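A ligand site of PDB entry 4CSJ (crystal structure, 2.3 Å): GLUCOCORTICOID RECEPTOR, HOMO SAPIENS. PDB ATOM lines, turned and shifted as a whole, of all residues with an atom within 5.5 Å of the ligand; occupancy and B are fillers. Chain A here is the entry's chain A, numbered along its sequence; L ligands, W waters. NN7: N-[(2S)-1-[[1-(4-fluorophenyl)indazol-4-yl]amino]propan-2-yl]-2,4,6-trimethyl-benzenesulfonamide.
OD1 of Asn 67 is in hydrogen-bond range of N22 of the ligand (2.7 Å). The backbone carbonyl oxygen (O) of Leu 66 is in hydrogen-bond range of a nitrogen (N5) of the ligand, 3.0 Å away. SG of Cys 239 lies close to O25 of the ligand. The side-chain amide nitrogen (NE2) of Gln 73 sits close to a nitrogen (N12) of the ligand.
The backbone carbonyl oxygen of Cys 239 lies within hydrogen-bond range of the side-chain hydroxyl of Thr 242 (3.1 Å). OE1 of Gln 145 lies close to SD of Met 63 (3.5 Å). The side-chain sulfur (SG) of Cys 146 lies within hydrogen-bond range of the backbone carbonyl oxygen (O) of Met 142 (3.4 Å). O of Tyr 238 sits close to OG1 of Thr 242.
The backbone carbonyl oxygen of Ala 110 lies close to a fluorine (F19) of the ligand, at 3.3 Å. NE of Arg 114 sits close to F19 of the ligand, 3.1 Å away. Met 63 touches the ligand. CD2 of Leu 69 touches N12 of the ligand, at 3.7 Å. N of Gly 70 touches C13 of the ligand, at 3.6 Å. Met 104 touches the ligand. Met 107 touches the ligand. N of Leu 111 touches C17 of the ligand (3.5 Å). Cys 125 touches the ligand. Phe 126 touches the ligand (O to C21, 3.1 Å). OE1 of Gln 145 touches C29 of the ligand, 3.4 Å away. SG of Cys 146 touches C31 of the ligand, 3.95 Å away. CE of Met 149 touches C32 of the ligand, at 3.6 Å. Leu 235 touches the ligand (CD2 to C34, 3.8 Å). OG1 of Thr 242 touches O24 of the ligand, 3.97 Å away. Leu 256 touches the ligand. Hydrophobic or aromatic side chains within 4 Å of the ligand: Met 63, Leu 66, Leu 69, Met 104, Met 107, Ala 110, Leu 111, Phe 126, Met 149, Leu 235 and Leu 256. Within 4 Å of the ligand: Met 63, Leu 66, Asn 67, Leu 69, Gly 70, Gln 73, Met 104, Met 107, Ala 110, Leu 111, Arg 114, Cys 125, Phe 126, Gln 145, Cys 146, Met 149, Leu 235, Cys 239, Thr 242 and Leu 256. Along chain A the residues within 4 Å of the ligand span positions 63 to 256. The nearest printed residue that does not touch the ligand is Phe 252 (4.01 Å).
Water W2 lies within hydrogen-bond range of an oxygen (O24) of the ligand, the side-chain hydroxyl of Thr 242 and the side-chain amide nitrogen of Asn 67.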
ATOM      1  N   MET A  63     -10.112  15.228  25.189  1.00  0.00           N
ATOM      2  CA  MET A  63     -11.107  15.448  26.222  1.00  0.00           C
ATOM      3  C   MET A  63     -10.873  16.760  26.938  1.00  0.00           C
ATOM      4  O   MET A  63     -11.801  17.547  27.066  1.00  0.00           O
ATOM      5  CB  MET A  63     -11.153  14.268  27.204  1.00  0.00           C
ATOM      6  CG  MET A  63     -11.802  13.021  26.644  1.00  0.00           C
ATOM      7  SD  MET A  63     -11.734  11.651  27.850  1.00  0.00           S
ATOM      8  CE  MET A  63     -13.037  12.119  29.036  1.00  0.00           C
ATOM      9  N   THR A  64      -9.621  17.013  27.361  1.00  0.00           N
ATOM     10  CA  THR A  64      -9.217  18.249  28.057  1.00  0.00           C
ATOM     11  C   THR A  64      -9.552  19.494  27.226  1.00  0.00           C
ATOM     12  O   THR A  64     -10.187  20.416  27.743  1.00  0.00           O
ATOM     13  CB  THR A  64      -7.722  18.188  28.447  1.00  0.00           C
ATOM     14  OG1 THR A  64      -7.533  17.104  29.341  1.00  0.00           O
ATOM     15  CG2 THR A  64      -7.231  19.470  29.098  1.00  0.00           C
ATOM     16  N   LEU A  66     -11.677  19.681  24.659  1.00  0.00           N
ATOM     17  CA  LEU A  66     -13.128  19.772  24.475  1.00  0.00           C
ATOM     18  C   LEU A  66     -13.841  20.360  25.692  1.00  0.00           C
ATOM     19  O   LEU A  66     -14.793  21.113  25.533  1.00  0.00           O
ATOM     20  CB  LEU A  66     -13.756  18.434  24.036  1.00  0.00           C
ATOM     21  CG  LEU A  66     -13.413  17.949  22.632  1.00  0.00           C
ATOM     22  CD1 LEU A  66     -14.106  16.645  22.317  1.00  0.00           C
ATOM     23  CD2 LEU A  66     -13.740  18.994  21.607  1.00  0.00           C
ATOM     24  N   ASN A  67     -13.320  20.079  26.903  1.00  0.00           N
ATOM     25  CA  ASN A  67     -13.870  20.658  28.134  1.00  0.00           C
ATOM     26  C   ASN A  67     -13.635  22.154  28.164  1.00  0.00           C
ATOM     27  O   ASN A  67     -14.574  22.890  28.441  1.00  0.00           O
ATOM     28  CB  ASN A  67     -13.295  19.962  29.378  1.00  0.00           C
ATOM     29  CG  ASN A  67     -13.862  18.601  29.583  1.00  0.00           C
ATOM     30  OD1 ASN A  67     -14.802  18.194  28.910  1.00  0.00           O
ATOM     31  ND2 ASN A  67     -13.265  17.829  30.479  1.00  0.00           N
ATOM     32  N   LEU A  69     -13.038  24.098  25.516  1.00  0.00           N
ATOM     33  CA  LEU A  69     -13.878  24.594  24.436  1.00  0.00           C
ATOM     34  C   LEU A  69     -15.338  24.686  24.901  1.00  0.00           C
ATOM     35  O   LEU A  69     -16.002  25.697  24.658  1.00  0.00           O
ATOM     36  CB  LEU A  69     -13.756  23.688  23.171  1.00  0.00           C
ATOM     37  CG  LEU A  69     -14.614  24.087  21.940  1.00  0.00           C
ATOM     38  CD1 LEU A  69     -14.313  25.557  21.467  1.00  0.00           C
ATOM     39  CD2 LEU A  69     -14.490  23.058  20.821  1.00  0.00           C
ATOM     40  N   GLY A  70     -15.797  23.662  25.631  1.00  0.00           N
ATOM     41  CA  GLY A  70     -17.139  23.593  26.178  1.00  0.00           C
ATOM     42  C   GLY A  70     -17.511  24.745  27.079  1.00  0.00           C
ATOM     43  O   GLY A  70     -18.650  25.224  27.031  1.00  0.00           O
ATOM     44  N   GLN A  73     -18.193  27.699  24.830  1.00  0.00           N
ATOM     45  CA  GLN A  73     -19.476  27.529  24.155  1.00  0.00           C
ATOM     46  C   GLN A  73     -20.599  27.910  25.111  1.00  0.00           C
ATOM     47  O   GLN A  73     -21.559  28.548  24.682  1.00  0.00           O
ATOM     48  CB  GLN A  73     -19.681  26.081  23.666  1.00  0.00           C
ATOM     49  CG  GLN A  73     -18.552  25.493  22.796  1.00  0.00           C
ATOM     50  CD  GLN A  73     -18.536  25.945  21.345  1.00  0.00           C
ATOM     51  OE1 GLN A  73     -19.068  26.988  20.956  1.00  0.00           O
ATOM     52  NE2 GLN A  73     -17.914  25.154  20.495  1.00  0.00           N
ATOM     53  N   TRP A 103     -27.861  22.823  29.172  1.00  0.00           N
ATOM     54  CA  TRP A 103     -26.504  23.046  28.643  1.00  0.00           C
ATOM     55  C   TRP A 103     -25.999  21.949  27.676  1.00  0.00           C
ATOM     56  O   TRP A 103     -25.653  22.281  26.537  1.00  0.00           O
ATOM     57  CB  TRP A 103     -25.503  23.286  29.780  1.00  0.00           C
ATOM     58  CG  TRP A 103     -25.093  22.069  30.545  1.00  0.00           C
ATOM     59  CD1 TRP A 103     -25.827  21.379  31.467  1.00  0.00           C
ATOM     60  CD2 TRP A 103     -23.813  21.422  30.482  1.00  0.00           C
ATOM     61  NE1 TRP A 103     -25.096  20.339  31.967  1.00  0.00           N
ATOM     62  CE2 TRP A 103     -23.831  20.367  31.427  1.00  0.00           C
ATOM     63  CE3 TRP A 103     -22.655  21.624  29.728  1.00  0.00           C
ATOM     64  CZ2 TRP A 103     -22.742  19.523  31.627  1.00  0.00           C
ATOM     65  CZ3 TRP A 103     -21.570  20.774  29.921  1.00  0.00           C
ATOM     66  CH2 TRP A 103     -21.623  19.742  30.867  1.00  0.00           C
ATOM     67  N   MET A 104     -26.001  20.660  28.095  1.00  0.00           N
ATOM     68  CA  MET A 104     -25.515  19.549  27.266  1.00  0.00           C
ATOM     69  C   MET A 104     -26.439  19.249  26.077  1.00  0.00           C
ATOM     70  O   MET A 104     -25.961  18.877  25.014  1.00  0.00           O
ATOM     71  CB  MET A 104     -25.236  18.281  28.120  1.00  0.00           C
ATOM     72  CG  MET A 104     -24.551  17.136  27.361  1.00  0.00           C
ATOM     73  SD  MET A 104     -22.925  17.529  26.634  1.00  0.00           S
ATOM     74  CE  MET A 104     -21.877  17.418  28.084  1.00  0.00           C
ATOM     75  N   LEU A 106     -28.275  21.569  24.459  1.00  0.00           N
ATOM     76  CA  LEU A 106     -27.966  22.658  23.531  1.00  0.00           C
ATOM     77  C   LEU A 106     -26.681  22.351  22.748  1.00  0.00           C
ATOM     78  O   LEU A 106     -26.675  22.405  21.511  1.00  0.00           O
ATOM     79  CB  LEU A 106     -27.817  24.004  24.282  1.00  0.00           C
ATOM     80  CG  LEU A 106     -29.068  24.541  25.008  1.00  0.00           C
ATOM     81  CD1 LEU A 106     -28.738  25.787  25.796  1.00  0.00           C
ATOM     82  CD2 LEU A 106     -30.202  24.820  24.024  1.00  0.00           C
ATOM     83  N   MET A 107     -25.626  21.949  23.481  1.00  0.00           N
ATOM     84  CA  MET A 107     -24.313  21.671  22.915  1.00  0.00           C
ATOM     85  C   MET A 107     -24.289  20.475  21.981  1.00  0.00           C
ATOM     86  O   MET A 107     -23.728  20.577  20.883  1.00  0.00           O
ATOM     87  CB  MET A 107     -23.267  21.549  24.017  1.00  0.00           C
ATOM     88  CG  MET A 107     -22.969  22.911  24.669  1.00  0.00           C
ATOM     89  SD  MET A 107     -21.289  23.103  25.225  1.00  0.00           S
ATOM     90  CE  MET A 107     -21.152  21.716  26.333  1.00  0.00           C
ATOM     91  N   ALA A 108     -24.904  19.345  22.375  1.00  0.00           N
ATOM     92  CA  ALA A 108     -24.976  18.180  21.498  1.00  0.00           C
ATOM     93  C   ALA A 108     -25.846  18.480  20.258  1.00  0.00           C
ATOM     94  O   ALA A 108     -25.504  18.041  19.159  1.00  0.00           O
ATOM     95  CB  ALA A 108     -25.526  16.984  22.255  1.00  0.00           C
ATOM     96  N   ALA A 110     -26.485  21.638  18.815  1.00  0.00           N
ATOM     97  CA  ALA A 110     -25.695  22.567  18.002  1.00  0.00           C
ATOM     98  C   ALA A 110     -24.537  21.833  17.281  1.00  0.00           C
ATOM     99  O   ALA A 110     -24.303  22.071  16.085  1.00  0.00           O
ATOM    100  CB  ALA A 110     -25.161  23.721  18.864  1.00  0.00           C
ATOM    101  N   LEU A 111     -23.864  20.901  17.982  1.00  0.00           N
ATOM    102  CA  LEU A 111     -22.777  20.112  17.406  1.00  0.00           C
ATOM    103  C   LEU A 111     -23.271  19.140  16.323  1.00  0.00           C
ATOM    104  O   LEU A 111     -22.623  18.992  15.286  1.00  0.00           O
ATOM    105  CB  LEU A 111     -22.009  19.372  18.504  1.00  0.00           C
ATOM    106  CG  LEU A 111     -21.034  18.269  18.044  1.00  0.00           C
ATOM    107  CD1 LEU A 111     -19.791  18.873  17.402  1.00  0.00           C
ATOM    108  CD2 LEU A 111     -20.673  17.375  19.194  1.00  0.00           C
ATOM    109  N   ARG A 114     -23.986  21.285  13.289  1.00  0.00           N
ATOM    110  CA  ARG A 114     -22.723  21.694  12.700  1.00  0.00           C
ATOM    111  C   ARG A 114     -22.046  20.533  12.003  1.00  0.00           C
ATOM    112  O   ARG A 114     -21.441  20.738  10.965  1.00  0.00           O
ATOM    113  CB  ARG A 114     -21.804  22.363  13.722  1.00  0.00           C
ATOM    114  CG  ARG A 114     -20.835  23.327  13.049  1.00  0.00           C
ATOM    115  CD  ARG A 114     -19.961  24.034  14.021  1.00  0.00           C
ATOM    116  NE  ARG A 114     -20.679  25.077  14.756  1.00  0.00           N
ATOM    117  CZ  ARG A 114     -20.133  25.781  15.749  1.00  0.00           C
ATOM    118  NH1 ARG A 114     -18.868  25.572  16.097  1.00  0.00           N
ATOM    119  NH2 ARG A 114     -20.836  26.694  16.384  1.00  0.00           N
ATOM    120  N   CYS A 125     -17.747  17.696  14.240  1.00  0.00           N
ATOM    121  CA  CYS A 125     -17.096  18.955  13.972  1.00  0.00           C
ATOM    122  C   CYS A 125     -17.224  19.907  15.173  1.00  0.00           C
ATOM    123  O   CYS A 125     -17.983  20.877  15.135  1.00  0.00           O
ATOM    124  CB  CYS A 125     -17.631  19.573  12.671  1.00  0.00           C
ATOM    125  SG  CYS A 125     -17.461  18.478  11.222  1.00  0.00           S
ATOM    126  N   PHE A 126     -16.469  19.595  16.247  1.00  0.00           N
ATOM    127  CA  PHE A 126     -16.450  20.406  17.483  1.00  0.00           C
ATOM    128  C   PHE A 126     -15.933  21.812  17.182  1.00  0.00           C
ATOM    129  O   PHE A 126     -16.446  22.791  17.710  1.00  0.00           O
ATOM    130  CB  PHE A 126     -15.557  19.746  18.541  1.00  0.00           C
ATOM    131  CG  PHE A 126     -16.206  18.571  19.237  1.00  0.00           C
ATOM    132  CD1 PHE A 126     -17.050  18.763  20.322  1.00  0.00           C
ATOM    133  CD2 PHE A 126     -15.959  17.274  18.804  1.00  0.00           C
ATOM    134  CE1 PHE A 126     -17.612  17.674  20.995  1.00  0.00           C
ATOM    135  CE2 PHE A 126     -16.540  16.180  19.464  1.00  0.00           C
ATOM    136  CZ  PHE A 126     -17.376  16.387  20.545  1.00  0.00           C
ATOM    137  N   ALA A 127     -14.895  21.894  16.356  1.00  0.00           N
ATOM    138  CA  ALA A 127     -14.286  23.160  15.964  1.00  0.00           C
ATOM    139  C   ALA A 127     -13.635  22.960  14.569  1.00  0.00           C
ATOM    140  O   ALA A 127     -13.359  21.810  14.194  1.00  0.00           O
ATOM    141  CB  ALA A 127     -13.245  23.587  16.991  1.00  0.00           C
ATOM    142  N   MET A 142     -12.845   6.961  22.768  1.00  0.00           N
ATOM    143  CA  MET A 142     -13.381   8.013  21.901  1.00  0.00           C
ATOM    144  C   MET A 142     -14.769   7.674  21.328  1.00  0.00           C
ATOM    145  O   MET A 142     -15.705   8.429  21.574  1.00  0.00           O
ATOM    146  CB  MET A 142     -12.399   8.393  20.783  1.00  0.00           C
ATOM    147  CG  MET A 142     -12.637   9.776  20.194  1.00  0.00           C
ATOM    148  SD  MET A 142     -12.602  11.127  21.407  1.00  0.00           S
ATOM    149  CE  MET A 142     -10.846  11.159  21.826  1.00  0.00           C
ATOM    150  N   GLN A 145     -17.900   7.792  23.581  1.00  0.00           N
ATOM    151  CA  GLN A 145     -18.204   9.176  23.931  1.00  0.00           C
ATOM    152  C   GLN A 145     -18.862   9.896  22.743  1.00  0.00           C
ATOM    153  O   GLN A 145     -19.773  10.694  22.938  1.00  0.00           O
ATOM    154  CB  GLN A 145     -16.907   9.907  24.353  1.00  0.00           C
ATOM    155  CG  GLN A 145     -16.325   9.438  25.703  1.00  0.00           C
ATOM    156  CD  GLN A 145     -14.972  10.040  26.015  1.00  0.00           C
ATOM    157  OE1 GLN A 145     -14.823  11.229  26.297  1.00  0.00           O
ATOM    158  NE2 GLN A 145     -13.943   9.206  26.026  1.00  0.00           N
ATOM    159  N   CYS A 146     -18.430   9.580  21.516  1.00  0.00           N
ATOM    160  CA  CYS A 146     -18.891  10.192  20.276  1.00  0.00           C
ATOM    161  C   CYS A 146     -20.207   9.663  19.708  1.00  0.00           C
ATOM    162  O   CYS A 146     -20.902  10.427  19.034  1.00  0.00           O
ATOM    163  CB  CYS A 146     -17.794  10.091  19.227  1.00  0.00           C
ATOM    164  SG  CYS A 146     -16.370  11.145  19.559  1.00  0.00           S
ATOM    165  N   MET A 149     -23.750  11.481  20.059  1.00  0.00           N
ATOM    166  CA  MET A 149     -23.759  12.757  19.357  1.00  0.00           C
ATOM    167  C   MET A 149     -23.807  12.468  17.854  1.00  0.00           C
ATOM    168  O   MET A 149     -24.506  13.175  17.130  1.00  0.00           O
ATOM    169  CB  MET A 149     -22.553  13.624  19.759  1.00  0.00           C
ATOM    170  CG  MET A 149     -22.717  14.218  21.156  1.00  0.00           C
ATOM    171  SD  MET A 149     -21.280  15.101  21.855  1.00  0.00           S
ATOM    172  CE  MET A 149     -20.013  13.889  21.647  1.00  0.00           C
ATOM    173  N   LEU A 235     -24.544  11.246  27.803  1.00  0.00           N
ATOM    174  CA  LEU A 235     -23.399  12.161  27.770  1.00  0.00           C
ATOM    175  C   LEU A 235     -23.005  12.590  29.198  1.00  0.00           C
ATOM    176  O   LEU A 235     -21.828  12.626  29.519  1.00  0.00           O
ATOM    177  CB  LEU A 235     -23.650  13.372  26.862  1.00  0.00           C
ATOM    178  CG  LEU A 235     -23.902  13.090  25.371  1.00  0.00           C
ATOM    179  CD1 LEU A 235     -24.348  14.352  24.647  1.00  0.00           C
ATOM    180  CD2 LEU A 235     -22.682  12.477  24.684  1.00  0.00           C
ATOM    181  N   TYR A 238     -20.682  10.079  31.413  1.00  0.00           N
ATOM    182  CA  TYR A 238     -19.234  10.203  31.173  1.00  0.00           C
ATOM    183  C   TYR A 238     -18.724  11.520  31.783  1.00  0.00           C
ATOM    184  O   TYR A 238     -17.716  11.531  32.494  1.00  0.00           O
ATOM    185  CB  TYR A 238     -18.897  10.135  29.662  1.00  0.00           C
ATOM    186  CG  TYR A 238     -19.396   8.882  28.963  1.00  0.00           C
ATOM    187  CD1 TYR A 238     -19.187   7.614  29.514  1.00  0.00           C
ATOM    188  CD2 TYR A 238     -20.036   8.964  27.732  1.00  0.00           C
ATOM    189  CE1 TYR A 238     -19.642   6.465  28.874  1.00  0.00           C
ATOM    190  CE2 TYR A 238     -20.508   7.816  27.085  1.00  0.00           C
ATOM    191  CZ  TYR A 238     -20.299   6.559  27.656  1.00  0.00           C
ATOM    192  OH  TYR A 238     -20.750   5.430  27.025  1.00  0.00           O
ATOM    193  N   CYS A 239     -19.448  12.622  31.527  1.00  0.00           N
ATOM    194  CA  CYS A 239     -19.127  13.949  32.022  1.00  0.00           C
ATOM    195  C   CYS A 239     -19.017  13.979  33.565  1.00  0.00           C
ATOM    196  O   CYS A 239     -18.006  14.441  34.093  1.00  0.00           O
ATOM    197  CB  CYS A 239     -20.154  14.960  31.517  1.00  0.00           C
ATOM    198  SG  CYS A 239     -19.856  16.643  32.082  1.00  0.00           S
ATOM    199  N   THR A 242     -15.866  11.762  34.938  1.00  0.00           N
ATOM    200  CA  THR A 242     -14.576  12.427  34.718  1.00  0.00           C
ATOM    201  C   THR A 242     -14.410  13.662  35.582  1.00  0.00           C
ATOM    202  O   THR A 242     -13.281  14.029  35.950  1.00  0.00           O
ATOM    203  CB  THR A 242     -14.355  12.755  33.225  1.00  0.00           C
ATOM    204  OG1 THR A 242     -15.290  13.748  32.811  1.00  0.00           O
ATOM    205  CG2 THR A 242     -14.499  11.530  32.340  1.00  0.00           C
ATOM    206  N   PHE A 252     -11.979  20.779  34.026  1.00  0.00           N
ATOM    207  CA  PHE A 252     -13.169  21.440  33.552  1.00  0.00           C
ATOM    208  C   PHE A 252     -13.007  22.925  33.863  1.00  0.00           C
ATOM    209  O   PHE A 252     -12.535  23.259  34.954  1.00  0.00           O
ATOM    210  CB  PHE A 252     -14.452  20.879  34.210  1.00  0.00           C
ATOM    211  CG  PHE A 252     -14.911  19.563  33.626  1.00  0.00           C
ATOM    212  CD1 PHE A 252     -14.326  18.366  34.030  1.00  0.00           C
ATOM    213  CD2 PHE A 252     -15.902  19.527  32.655  1.00  0.00           C
ATOM    214  CE1 PHE A 252     -14.754  17.148  33.504  1.00  0.00           C
ATOM    215  CE2 PHE A 252     -16.347  18.308  32.140  1.00  0.00           C
ATOM    216  CZ  PHE A 252     -15.775  17.129  32.563  1.00  0.00           C
ATOM    217  N   LEU A 256     -18.127  25.253  33.390  1.00  0.00           N
ATOM    218  CA  LEU A 256     -18.640  23.896  33.417  1.00  0.00           C
ATOM    219  C   LEU A 256     -18.610  23.324  34.800  1.00  0.00           C
ATOM    220  O   LEU A 256     -19.580  22.678  35.177  1.00  0.00           O
ATOM    221  CB  LEU A 256     -17.953  22.995  32.380  1.00  0.00           C
ATOM    222  CG  LEU A 256     -18.091  23.443  30.907  1.00  0.00           C
ATOM    223  CD1 LEU A 256     -17.518  22.422  29.979  1.00  0.00           C
ATOM    224  CD2 LEU A 256     -19.547  23.800  30.529  1.00  0.00           C
HETATM  225  C1  NN7 L   1     -18.123  19.392  28.297  1.00  0.00           C
HETATM  226  C2  NN7 L   1     -17.899  18.094  27.505  1.00  0.00           C
HETATM  227  C4  NN7 L   1     -16.967  18.270  26.289  1.00  0.00           C
HETATM  228  N5  NN7 L   1     -17.297  19.432  25.439  1.00  0.00           N
HETATM  229  C6  NN7 L   1     -18.331  19.459  24.481  1.00  0.00           C
HETATM  230  C7  NN7 L   1     -19.411  18.584  24.471  1.00  0.00           C
HETATM  231  C8  NN7 L   1     -20.445  18.701  23.538  1.00  0.00           C
HETATM  232  C9  NN7 L   1     -20.411  19.667  22.557  1.00  0.00           C
HETATM  233  C10 NN7 L   1     -19.324  20.567  22.542  1.00  0.00           C
HETATM  234  N11 NN7 L   1     -18.990  21.624  21.727  1.00  0.00           N
HETATM  235  N12 NN7 L   1     -17.788  22.152  22.189  1.00  0.00           N
HETATM  236  C13 NN7 L   1     -17.347  21.480  23.219  1.00  0.00           C
HETATM  237  C14 NN7 L   1     -18.286  20.468  23.501  1.00  0.00           C
HETATM  238  C15 NN7 L   1     -19.703  22.097  20.622  1.00  0.00           C
HETATM  239  C16 NN7 L   1     -21.019  22.565  20.743  1.00  0.00           C
HETATM  240  C17 NN7 L   1     -21.674  23.025  19.615  1.00  0.00           C
HETATM  241  C18 NN7 L   1     -21.005  23.106  18.387  1.00  0.00           C
HETATM  242  F19 NN7 L   1     -21.666  23.552  17.303  1.00  0.00           F
HETATM  243  C20 NN7 L   1     -19.681  22.689  18.262  1.00  0.00           C
HETATM  244  C21 NN7 L   1     -19.037  22.172  19.386  1.00  0.00           C
HETATM  245  N22 NN7 L   1     -17.284  17.123  28.430  1.00  0.00           N
HETATM  246  S23 NN7 L   1     -17.703  15.523  28.379  1.00  0.00           S
HETATM  247  O24 NN7 L   1     -16.857  14.873  29.343  1.00  0.00           O
HETATM  248  O25 NN7 L   1     -19.115  15.538  28.537  1.00  0.00           O
HETATM  249  C26 NN7 L   1     -17.294  14.852  26.763  1.00  0.00           C
HETATM  250  C27 NN7 L   1     -15.967  14.799  26.314  1.00  0.00           C
HETATM  251  C28 NN7 L   1     -14.783  15.251  27.137  1.00  0.00           C
HETATM  252  C29 NN7 L   1     -15.640  14.320  25.056  1.00  0.00           C
HETATM  253  C30 NN7 L   1     -16.628  13.902  24.191  1.00  0.00           C
HETATM  254  C31 NN7 L   1     -16.257  13.366  22.827  1.00  0.00           C
HETATM  255  C32 NN7 L   1     -17.952  13.907  24.621  1.00  0.00           C
HETATM  256  C33 NN7 L   1     -18.287  14.386  25.885  1.00  0.00           C
HETATM  257  C34 NN7 L   1     -19.773  14.449  26.174  1.00  0.00           C
HETATM  258  O   HOH W   1     -23.192  25.113  21.503  1.00  0.00           O
HETATM  259  O   HOH W   2     -14.364  15.087  30.413  1.00  0.00           O
